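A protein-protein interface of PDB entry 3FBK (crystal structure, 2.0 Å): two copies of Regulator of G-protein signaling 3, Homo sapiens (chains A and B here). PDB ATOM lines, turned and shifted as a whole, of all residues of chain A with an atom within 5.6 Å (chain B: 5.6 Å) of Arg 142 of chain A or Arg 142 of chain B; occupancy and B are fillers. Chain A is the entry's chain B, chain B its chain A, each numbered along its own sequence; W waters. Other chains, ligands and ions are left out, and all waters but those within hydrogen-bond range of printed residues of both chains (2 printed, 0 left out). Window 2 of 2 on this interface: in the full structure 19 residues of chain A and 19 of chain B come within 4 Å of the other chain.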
ATOM      1  N   ILE A  56     -28.659  14.566  25.333  1.00  0.00           N
ATOM      2  CA  ILE A  56     -29.012  15.029  23.993  1.00  0.00           C
ATOM      3  C   ILE A  56     -29.318  13.852  23.071  1.00  0.00           C
ATOM      4  O   ILE A  56     -28.729  12.777  23.202  1.00  0.00           O
ATOM      5  CB  ILE A  56     -27.876  15.858  23.342  1.00  0.00           C
ATOM      6  CG1 ILE A  56     -26.607  15.008  23.215  1.00  0.00           C
ATOM      7  CG2 ILE A  56     -27.604  17.108  24.176  1.00  0.00           C
ATOM      8  CD1 ILE A  56     -25.439  15.747  22.553  1.00  0.00           C
ATOM      9  N   ARG A  94     -27.361  10.720  24.469  1.00  0.00           N
ATOM     10  CA  ARG A  94     -25.973  10.768  24.887  1.00  0.00           C
ATOM     11  C   ARG A  94     -25.854  11.730  26.052  1.00  0.00           C
ATOM     12  O   ARG A  94     -26.553  12.743  26.109  1.00  0.00           O
ATOM     13  CB  ARG A  94     -25.072  11.224  23.726  1.00  0.00           C
ATOM     14  CG  ARG A  94     -25.095  10.308  22.502  1.00  0.00           C
ATOM     15  CD  ARG A  94     -24.151  10.818  21.409  1.00  0.00           C
ATOM     16  NE  ARG A  94     -22.761  10.878  21.866  1.00  0.00           N
ATOM     17  CZ  ARG A  94     -21.989   9.810  22.072  1.00  0.00           C
ATOM     18  NH1 ARG A  94     -22.463   8.583  21.856  1.00  0.00           N
ATOM     19  NH2 ARG A  94     -20.742   9.967  22.497  1.00  0.00           N
ATOM     20  N   LEU A  96     -24.067  14.531  27.657  1.00  0.00           N
ATOM     21  CA  LEU A  96     -23.170  15.602  27.229  1.00  0.00           C
ATOM     22  C   LEU A  96     -22.567  16.330  28.419  1.00  0.00           C
ATOM     23  O   LEU A  96     -23.285  16.719  29.338  1.00  0.00           O
ATOM     24  CB  LEU A  96     -23.943  16.606  26.368  1.00  0.00           C
ATOM     25  CG  LEU A  96     -23.187  17.771  25.717  1.00  0.00           C
ATOM     26  CD1 LEU A  96     -22.290  17.226  24.592  1.00  0.00           C
ATOM     27  CD2 LEU A  96     -24.175  18.790  25.132  1.00  0.00           C
ATOM     28  N   CYS A 114     -16.432  20.288  24.898  1.00  0.00           N
ATOM     29  CA  CYS A 114     -17.391  19.295  25.375  1.00  0.00           C
ATOM     30  C   CYS A 114     -17.019  17.867  24.969  1.00  0.00           C
ATOM     31  O   CYS A 114     -16.077  17.647  24.214  1.00  0.00           O
ATOM     32  CB  CYS A 114     -18.804  19.631  24.877  1.00  0.00           C
ATOM     33  SG  CYS A 114     -19.040  19.595  23.073  1.00  0.00           S
ATOM     34  N   MET A 115     -17.760  16.902  25.502  1.00  0.00           N
ATOM     35  CA  MET A 115     -17.540  15.487  25.206  1.00  0.00           C
ATOM     36  C   MET A 115     -18.858  14.816  25.536  1.00  0.00           C
ATOM     37  O   MET A 115     -19.697  15.402  26.209  1.00  0.00           O
ATOM     38  CB  MET A 115     -16.435  14.906  26.092  1.00  0.00           C
ATOM     39  CG  MET A 115     -16.731  14.985  27.579  1.00  0.00           C
ATOM     40  SD  MET A 115     -15.280  14.249  28.625  1.00  0.00           S
ATOM     41  CE  MET A 115     -14.207  15.848  28.760  1.00  0.00           C
ATOM     42  N   SER A 116     -19.050  13.597  25.061  1.00  0.00           N
ATOM     43  CA  SER A 116     -20.293  12.903  25.333  1.00  0.00           C
ATOM     44  C   SER A 116     -20.071  11.414  25.499  1.00  0.00           C
ATOM     45  O   SER A 116     -19.052  10.879  25.068  1.00  0.00           O
ATOM     46  CB  SER A 116     -21.302  13.174  24.212  1.00  0.00           C
ATOM     47  OG  SER A 116     -20.770  12.823  22.952  1.00  0.00           O
ATOM     48  N   GLY A 137     -14.457  20.009  20.299  1.00  0.00           N
ATOM     49  CA  GLY A 137     -15.211  21.130  19.762  1.00  0.00           C
ATOM     50  C   GLY A 137     -16.715  20.993  19.922  1.00  0.00           C
ATOM     51  O   GLY A 137     -17.232  19.895  20.160  1.00  0.00           O
ATOM     52  N   GLU A 138     -17.416  22.117  19.777  1.00  0.00           N
ATOM     53  CA  GLU A 138     -18.874  22.184  19.904  1.00  0.00           C
ATOM     54  C   GLU A 138     -19.661  21.182  19.052  1.00  0.00           C
ATOM     55  O   GLU A 138     -20.818  20.866  19.367  1.00  0.00           O
ATOM     56  CB  GLU A 138     -19.358  23.597  19.569  1.00  0.00           C
ATOM     57  CG  GLU A 138     -19.154  23.985  18.116  1.00  0.00           C
ATOM     58  CD  GLU A 138     -19.303  25.474  17.877  1.00  0.00           C
ATOM     59  OE1 GLU A 138     -20.418  26.003  18.066  1.00  0.00           O
ATOM     60  OE2 GLU A 138     -18.297  26.114  17.506  1.00  0.00           O
ATOM     61  N   HIS A 139     -19.065  20.705  17.962  1.00  0.00           N
ATOM     62  CA  HIS A 139     -19.754  19.731  17.122  1.00  0.00           C
ATOM     63  C   HIS A 139     -19.225  18.331  17.422  1.00  0.00           C
ATOM     64  O   HIS A 139     -19.985  17.442  17.784  1.00  0.00           O
ATOM     65  CB  HIS A 139     -19.570  20.068  15.637  1.00  0.00           C
ATOM     66  CG  HIS A 139     -20.087  21.423  15.267  1.00  0.00           C
ATOM     67  ND1 HIS A 139     -19.346  22.335  14.546  1.00  0.00           N
ATOM     68  CD2 HIS A 139     -21.254  22.046  15.569  1.00  0.00           C
ATOM     69  CE1 HIS A 139     -20.029  23.459  14.423  1.00  0.00           C
ATOM     70  NE2 HIS A 139     -21.191  23.310  15.036  1.00  0.00           N
ATOM     71  N   LEU A 140     -17.917  18.144  17.302  1.00  0.00           N
ATOM     72  CA  LEU A 140     -17.310  16.838  17.552  1.00  0.00           C
ATOM     73  C   LEU A 140     -17.634  16.259  18.931  1.00  0.00           C
ATOM     74  O   LEU A 140     -17.906  15.061  19.067  1.00  0.00           O
ATOM     75  CB  LEU A 140     -15.793  16.931  17.394  1.00  0.00           C
ATOM     76  CG  LEU A 140     -15.046  15.607  17.568  1.00  0.00           C
ATOM     77  CD1 LEU A 140     -15.449  14.646  16.455  1.00  0.00           C
ATOM     78  CD2 LEU A 140     -13.542  15.851  17.543  1.00  0.00           C
ATOM     79  N   GLY A 141     -17.607  17.111  19.956  1.00  0.00           N
ATOM     80  CA  GLY A 141     -17.880  16.648  21.308  1.00  0.00           C
ATOM     81  C   GLY A 141     -19.245  16.028  21.562  1.00  0.00           C
ATOM     82  O   GLY A 141     -19.427  15.297  22.537  1.00  0.00           O
ATOM     83  N   ARG A 142     -20.209  16.322  20.697  1.00  0.00           N
ATOM     84  CA  ARG A 142     -21.560  15.791  20.851  1.00  0.00           C
ATOM     85  C   ARG A 142     -21.647  14.397  20.250  1.00  0.00           C
ATOM     86  O   ARG A 142     -22.683  13.736  20.351  1.00  0.00           O
ATOM     87  CB  ARG A 142     -22.578  16.690  20.137  1.00  0.00           C
ATOM     88  CG  ARG A 142     -22.563  18.158  20.576  1.00  0.00           C
ATOM     89  CD  ARG A 142     -23.489  19.004  19.697  1.00  0.00           C
ATOM     90  NE  ARG A 142     -24.909  18.770  19.970  1.00  0.00           N
ATOM     91  CZ  ARG A 142     -25.576  19.310  20.984  1.00  0.00           C
ATOM     92  NH1 ARG A 142     -26.865  19.042  21.151  1.00  0.00           N
ATOM     93  NH2 ARG A 142     -24.959  20.124  21.834  1.00  0.00           N
ATOM     94  N   THR A 143     -20.555  13.944  19.641  1.00  0.00           N
ATOM     95  CA  THR A 143     -20.540  12.645  18.981  1.00  0.00           C
ATOM     96  C   THR A 143     -19.665  11.590  19.627  1.00  0.00           C
ATOM     97  O   THR A 143     -19.827  10.408  19.344  1.00  0.00           O
ATOM     98  CB  THR A 143     -20.067  12.778  17.514  1.00  0.00           C
ATOM     99  OG1 THR A 143     -18.662  13.069  17.487  1.00  0.00           O
ATOM    100  CG2 THR A 143     -20.820  13.891  16.811  1.00  0.00           C
ATOM    101  N   LYS A 144     -18.739  12.006  20.486  1.00  0.00           N
ATOM    102  CA  LYS A 144     -17.837  11.040  21.104  1.00  0.00           C
ATOM    103  C   LYS A 144     -17.086  11.649  22.265  1.00  0.00           C
ATOM    104  O   LYS A 144     -17.363  12.757  22.680  1.00  0.00           O
ATOM    105  CB  LYS A 144     -16.811  10.576  20.072  1.00  0.00           C
ATOM    106  CG  LYS A 144     -15.859  11.692  19.604  1.00  0.00           C
ATOM    107  CD  LYS A 144     -14.864  11.191  18.546  1.00  0.00           C
ATOM    108  CE  LYS A 144     -13.931  10.098  19.088  1.00  0.00           C
ATOM    109  NZ  LYS A 144     -14.608   8.822  19.501  1.00  0.00           N
ATOM    110  N   ILE B  56     -26.949  28.699  18.528  1.00  0.00           N
ATOM    111  CA  ILE B  56     -25.966  27.824  19.156  1.00  0.00           C
ATOM    112  C   ILE B  56     -24.546  28.259  18.819  1.00  0.00           C
ATOM    113  O   ILE B  56     -24.287  28.763  17.728  1.00  0.00           O
ATOM    114  CB  ILE B  56     -26.129  26.349  18.712  1.00  0.00           C
ATOM    115  CG1 ILE B  56     -25.936  26.228  17.201  1.00  0.00           C
ATOM    116  CG2 ILE B  56     -27.508  25.828  19.115  1.00  0.00           C
ATOM    117  CD1 ILE B  56     -26.054  24.799  16.682  1.00  0.00           C
ATOM    118  N   ARG B  94     -24.685  30.168  15.367  1.00  0.00           N
ATOM    119  CA  ARG B  94     -25.419  29.688  14.214  1.00  0.00           C
ATOM    120  C   ARG B  94     -26.890  29.625  14.581  1.00  0.00           C
ATOM    121  O   ARG B  94     -27.255  29.326  15.723  1.00  0.00           O
ATOM    122  CB  ARG B  94     -24.918  28.303  13.793  1.00  0.00           C
ATOM    123  CG  ARG B  94     -23.445  28.256  13.388  1.00  0.00           C
ATOM    124  CD  ARG B  94     -23.038  26.836  12.966  1.00  0.00           C
ATOM    125  NE  ARG B  94     -23.805  26.363  11.810  1.00  0.00           N
ATOM    126  CZ  ARG B  94     -23.659  26.822  10.566  1.00  0.00           C
ATOM    127  NH1 ARG B  94     -22.764  27.769  10.296  1.00  0.00           N
ATOM    128  NH2 ARG B  94     -24.422  26.349   9.590  1.00  0.00           N
ATOM    129  N   LEU B  96     -30.082  27.757  14.544  1.00  0.00           N
ATOM    130  CA  LEU B  96     -30.473  26.357  14.421  1.00  0.00           C
ATOM    131  C   LEU B  96     -31.984  26.230  14.239  1.00  0.00           C
ATOM    132  O   LEU B  96     -32.755  26.856  14.962  1.00  0.00           O
ATOM    133  CB  LEU B  96     -30.045  25.585  15.679  1.00  0.00           C
ATOM    134  CG  LEU B  96     -30.271  24.067  15.736  1.00  0.00           C
ATOM    135  CD1 LEU B  96     -29.323  23.384  14.757  1.00  0.00           C
ATOM    136  CD2 LEU B  96     -29.999  23.541  17.158  1.00  0.00           C
ATOM    137  N   CYS B 114     -32.596  18.600  11.585  1.00  0.00           N
ATOM    138  CA  CYS B 114     -32.256  20.000  11.795  1.00  0.00           C
ATOM    139  C   CYS B 114     -31.319  20.552  10.722  1.00  0.00           C
ATOM    140  O   CYS B 114     -30.844  19.831   9.850  1.00  0.00           O
ATOM    141  CB  CYS B 114     -31.636  20.197  13.183  1.00  0.00           C
ATOM    142  SG  CYS B 114     -30.054  19.369  13.473  1.00  0.00           S
ATOM    143  N   MET B 115     -31.094  21.858  10.776  1.00  0.00           N
ATOM    144  CA  MET B 115     -30.223  22.549   9.823  1.00  0.00           C
ATOM    145  C   MET B 115     -29.814  23.830  10.514  1.00  0.00           C
ATOM    146  O   MET B 115     -30.446  24.234  11.474  1.00  0.00           O
ATOM    147  CB  MET B 115     -30.979  22.878   8.530  1.00  0.00           C
ATOM    148  CG  MET B 115     -32.180  23.796   8.732  1.00  0.00           C
ATOM    149  SD  MET B 115     -33.128  24.185   7.093  1.00  0.00           S
ATOM    150  CE  MET B 115     -34.210  22.599   7.044  1.00  0.00           C
ATOM    151  N   SER B 116     -28.768  24.478  10.026  1.00  0.00           N
ATOM    152  CA  SER B 116     -28.325  25.704  10.657  1.00  0.00           C
ATOM    153  C   SER B 116     -27.786  26.687   9.637  1.00  0.00           C
ATOM    154  O   SER B 116     -27.421  26.308   8.529  1.00  0.00           O
ATOM    155  CB  SER B 116     -27.267  25.397  11.719  1.00  0.00           C
ATOM    156  OG  SER B 116     -26.180  24.697  11.172  1.00  0.00           O
ATOM    157  N   GLY B 137     -29.142  15.335   9.970  1.00  0.00           N
ATOM    158  CA  GLY B 137     -29.034  14.641  11.244  1.00  0.00           C
ATOM    159  C   GLY B 137     -28.711  15.550  12.412  1.00  0.00           C
ATOM    160  O   GLY B 137     -28.249  16.682  12.223  1.00  0.00           O
ATOM    161  N   GLU B 138     -28.946  15.041  13.623  1.00  0.00           N
ATOM    162  CA  GLU B 138     -28.710  15.777  14.867  1.00  0.00           C
ATOM    163  C   GLU B 138     -27.314  16.384  15.018  1.00  0.00           C
ATOM    164  O   GLU B 138     -27.132  17.337  15.782  1.00  0.00           O
ATOM    165  CB  GLU B 138     -28.985  14.876  16.073  1.00  0.00           C
ATOM    166  CG  GLU B 138     -28.004  13.723  16.205  1.00  0.00           C
ATOM    167  CD  GLU B 138     -28.481  12.645  17.159  1.00  0.00           C
ATOM    168  OE1 GLU B 138     -28.610  12.921  18.368  1.00  0.00           O
ATOM    169  OE2 GLU B 138     -28.735  11.515  16.694  1.00  0.00           O
ATOM    170  N   HIS B 139     -26.324  15.825  14.331  1.00  0.00           N
ATOM    171  CA  HIS B 139     -24.974  16.375  14.413  1.00  0.00           C
ATOM    172  C   HIS B 139     -24.683  17.241  13.190  1.00  0.00           C
ATOM    173  O   HIS B 139     -24.358  18.415  13.321  1.00  0.00           O
ATOM    174  CB  HIS B 139     -23.940  15.251  14.530  1.00  0.00           C
ATOM    175  CG  HIS B 139     -24.150  14.374  15.728  1.00  0.00           C
ATOM    176  ND1 HIS B 139     -24.180  12.995  15.650  1.00  0.00           N
ATOM    177  CD2 HIS B 139     -24.395  14.684  17.021  1.00  0.00           C
ATOM    178  CE1 HIS B 139     -24.442  12.499  16.845  1.00  0.00           C
ATOM    179  NE2 HIS B 139     -24.580  13.495  17.695  1.00  0.00           N
ATOM    180  N   LEU B 140     -24.827  16.665  12.003  1.00  0.00           N
ATOM    181  CA  LEU B 140     -24.572  17.395  10.767  1.00  0.00           C
ATOM    182  C   LEU B 140     -25.358  18.704  10.635  1.00  0.00           C
ATOM    183  O   LEU B 140     -24.819  19.715  10.182  1.00  0.00           O
ATOM    184  CB  LEU B 140     -24.885  16.507   9.560  1.00  0.00           C
ATOM    185  CG  LEU B 140     -24.593  17.148   8.197  1.00  0.00           C
ATOM    186  CD1 LEU B 140     -23.093  17.400   8.067  1.00  0.00           C
ATOM    187  CD2 LEU B 140     -25.075  16.233   7.079  1.00  0.00           C
ATOM    188  N   GLY B 141     -26.627  18.677  11.026  1.00  0.00           N
ATOM    189  CA  GLY B 141     -27.471  19.859  10.911  1.00  0.00           C
ATOM    190  C   GLY B 141     -27.040  21.084  11.702  1.00  0.00           C
ATOM    191  O   GLY B 141     -27.462  22.208  11.393  1.00  0.00           O
ATOM    192  N   ARG B 142     -26.213  20.879  12.725  1.00  0.00           N
ATOM    193  CA  ARG B 142     -25.739  21.986  13.551  1.00  0.00           C
ATOM    194  C   ARG B 142     -24.538  22.646  12.887  1.00  0.00           C
ATOM    195  O   ARG B 142     -24.032  23.651  13.376  1.00  0.00           O
ATOM    196  CB  ARG B 142     -25.311  21.483  14.933  1.00  0.00           C
ATOM    197  CG  ARG B 142     -26.378  20.707  15.697  1.00  0.00           C
ATOM    198  CD  ARG B 142     -25.802  20.097  16.974  1.00  0.00           C
ATOM    199  NE  ARG B 142     -25.549  21.093  18.016  1.00  0.00           N
ATOM    200  CZ  ARG B 142     -26.487  21.605  18.809  1.00  0.00           C
ATOM    201  NH1 ARG B 142     -26.165  22.507  19.726  1.00  0.00           N
ATOM    202  NH2 ARG B 142     -27.747  21.206  18.697  1.00  0.00           N
ATOM    203  N   THR B 143     -24.095  22.086  11.765  1.00  0.00           N
ATOM    204  CA  THR B 143     -22.921  22.603  11.069  1.00  0.00           C
ATOM    205  C   THR B 143     -23.181  23.243   9.718  1.00  0.00           C
ATOM    206  O   THR B 143     -22.328  23.974   9.203  1.00  0.00           O
ATOM    207  CB  THR B 143     -21.877  21.486  10.839  1.00  0.00           C
ATOM    208  OG1 THR B 143     -22.346  20.589   9.822  1.00  0.00           O
ATOM    209  CG2 THR B 143     -21.642  20.715  12.113  1.00  0.00           C
ATOM    210  N   LYS B 144     -24.345  22.979   9.135  1.00  0.00           N
ATOM    211  CA  LYS B 144     -24.629  23.534   7.823  1.00  0.00           C
ATOM    212  C   LYS B 144     -26.088  23.384   7.458  1.00  0.00           C
ATOM    213  O   LYS B 144     -26.908  22.974   8.278  1.00  0.00           O
ATOM    214  CB  LYS B 144     -23.806  22.800   6.769  1.00  0.00           C
ATOM    215  CG  LYS B 144     -24.197  21.319   6.609  1.00  0.00           C
ATOM    216  CD  LYS B 144     -23.335  20.601   5.567  1.00  0.00           C
ATOM    217  CE  LYS B 144     -23.513  21.196   4.164  1.00  0.00           C
ATOM    218  NZ  LYS B 144     -23.065  22.623   4.006  1.00  0.00           N
HETATM  219  O   HOH W   1     -25.871  16.902  18.142  1.00  0.00           O
HETATM  220  O   HOH W   2     -22.768  21.891  17.864  1.00  0.00           O
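A ring nitrogen (NE2) of His 139 of chain B sits at hydrogen-bond distance from the backbone carbonyl oxygen (O) of Arg 142 of chain A (3.3 Å). NE2 of His 139 of chain A sits at hydrogen-bond distance from O of Arg 142 of chain B, 3.3 Å away. The guanidinium group (NE) of Arg 142 of chain A lies close to the guanidinium group (NE) of Arg 142 of chain B, 3.1 Å away.
OG of Ser 116 of chain B lies close to O of Arg 142 of chain B, at 3.3 Å. N of Thr 143 of chain B lies within hydrogen-bond range of OG of Ser 116 of chain B, at 3.4 Å. The guanidinium group (NE) of Arg 94 of chain A sits at hydrogen-bond distance from the backbone carbonyl oxygen (O) of Arg 142 of chain A, 3.2 Å away. NH2 of Arg 94 of chain A is in hydrogen-bond range of O of Thr 143 of chain A. O of Arg 142 of chain A sits close to OG of Ser 116 of chain A, at 3.4 Å. The backbone carbonyl oxygen (O) of Leu 140 of chain A sits at hydrogen-bond distance from the side-chain hydroxyl (OG1) of Thr 143 of chain A, 2.7 Å away.
Among the printed residues, merely in contact across the chains: His 139 of chain A with Thr 143 of chain B and Thr 143 of chain A with His 139 of chain B.
Of the printed residues of chain B, His 139 of chain A touches Arg 142 (3.3 Å) and Thr 143 (3.6 Å). Of chain B, only His 139 and Arg 142 come within 4 Å of Arg 142 of chain A. Of the printed residues of chain B, Thr 143 of chain A touches His 139 (3.5 Å). Ser 116 of chain B touches none of the printed residues of chain A. Gly 137 of chain B touches none of the printed residues of chain A. Of the printed residues of chain A, His 139 of chain B touches Arg 142 (3.3 Å) and Thr 143 (3.5 Å). Of the printed residues of chain A, Arg 142 of chain B touches His 139 and Arg 142. Of the printed residues of chain A, Thr 143 of chain B touches His 139 (3.6 Å). The nearest residue of chain A that does not touch Arg 142 of chain B is Glu 138 of chain A (4.9 Å).
Of the 14 printed residues of chain B, 3 touch a printed residue of chain A. Printed residues of chain B that touch a printed residue of chain A: His 139, Arg 142 and Thr 143. Hydrophobic or aromatic side chains of chain B that line the printed part of chain A: His 139. Of the 14 printed residues of chain A, 3 touch a printed residue of chain B. Among the printed residues, no Asp or Glu carboxylate lies within 4 Å of a Lys or Arg side-chain nitrogen of the other chain.
His 139 of chain A touches Arg 142 of chain B, and with the chains exchanged Arg 142 of chain A touches His 139 of chain B. His 139 of chain A touches Thr 143 of chain B, and with the chains exchanged Thr 143 of chain A touches His 139 of chain B. Arg 142 of chain A touches its own counterpart, Arg 142 of chain B. Positions printed for both chains: 56, 94, 96, 114, 115, 116, 137, 138, 139, 140, 141, 142, 143 and 144. Of the 5 pairs that touch across the chains among the printed residues, 5 have their exchanged pair printed and touching as well.
Water W2 bridges O of Glu 138 of chain A and NE of Arg 142 of chain B. Water W1 bridges O of Glu 138 of chain B (2.7 Å) and NE of Arg 142 of chain A (2.8 Å).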
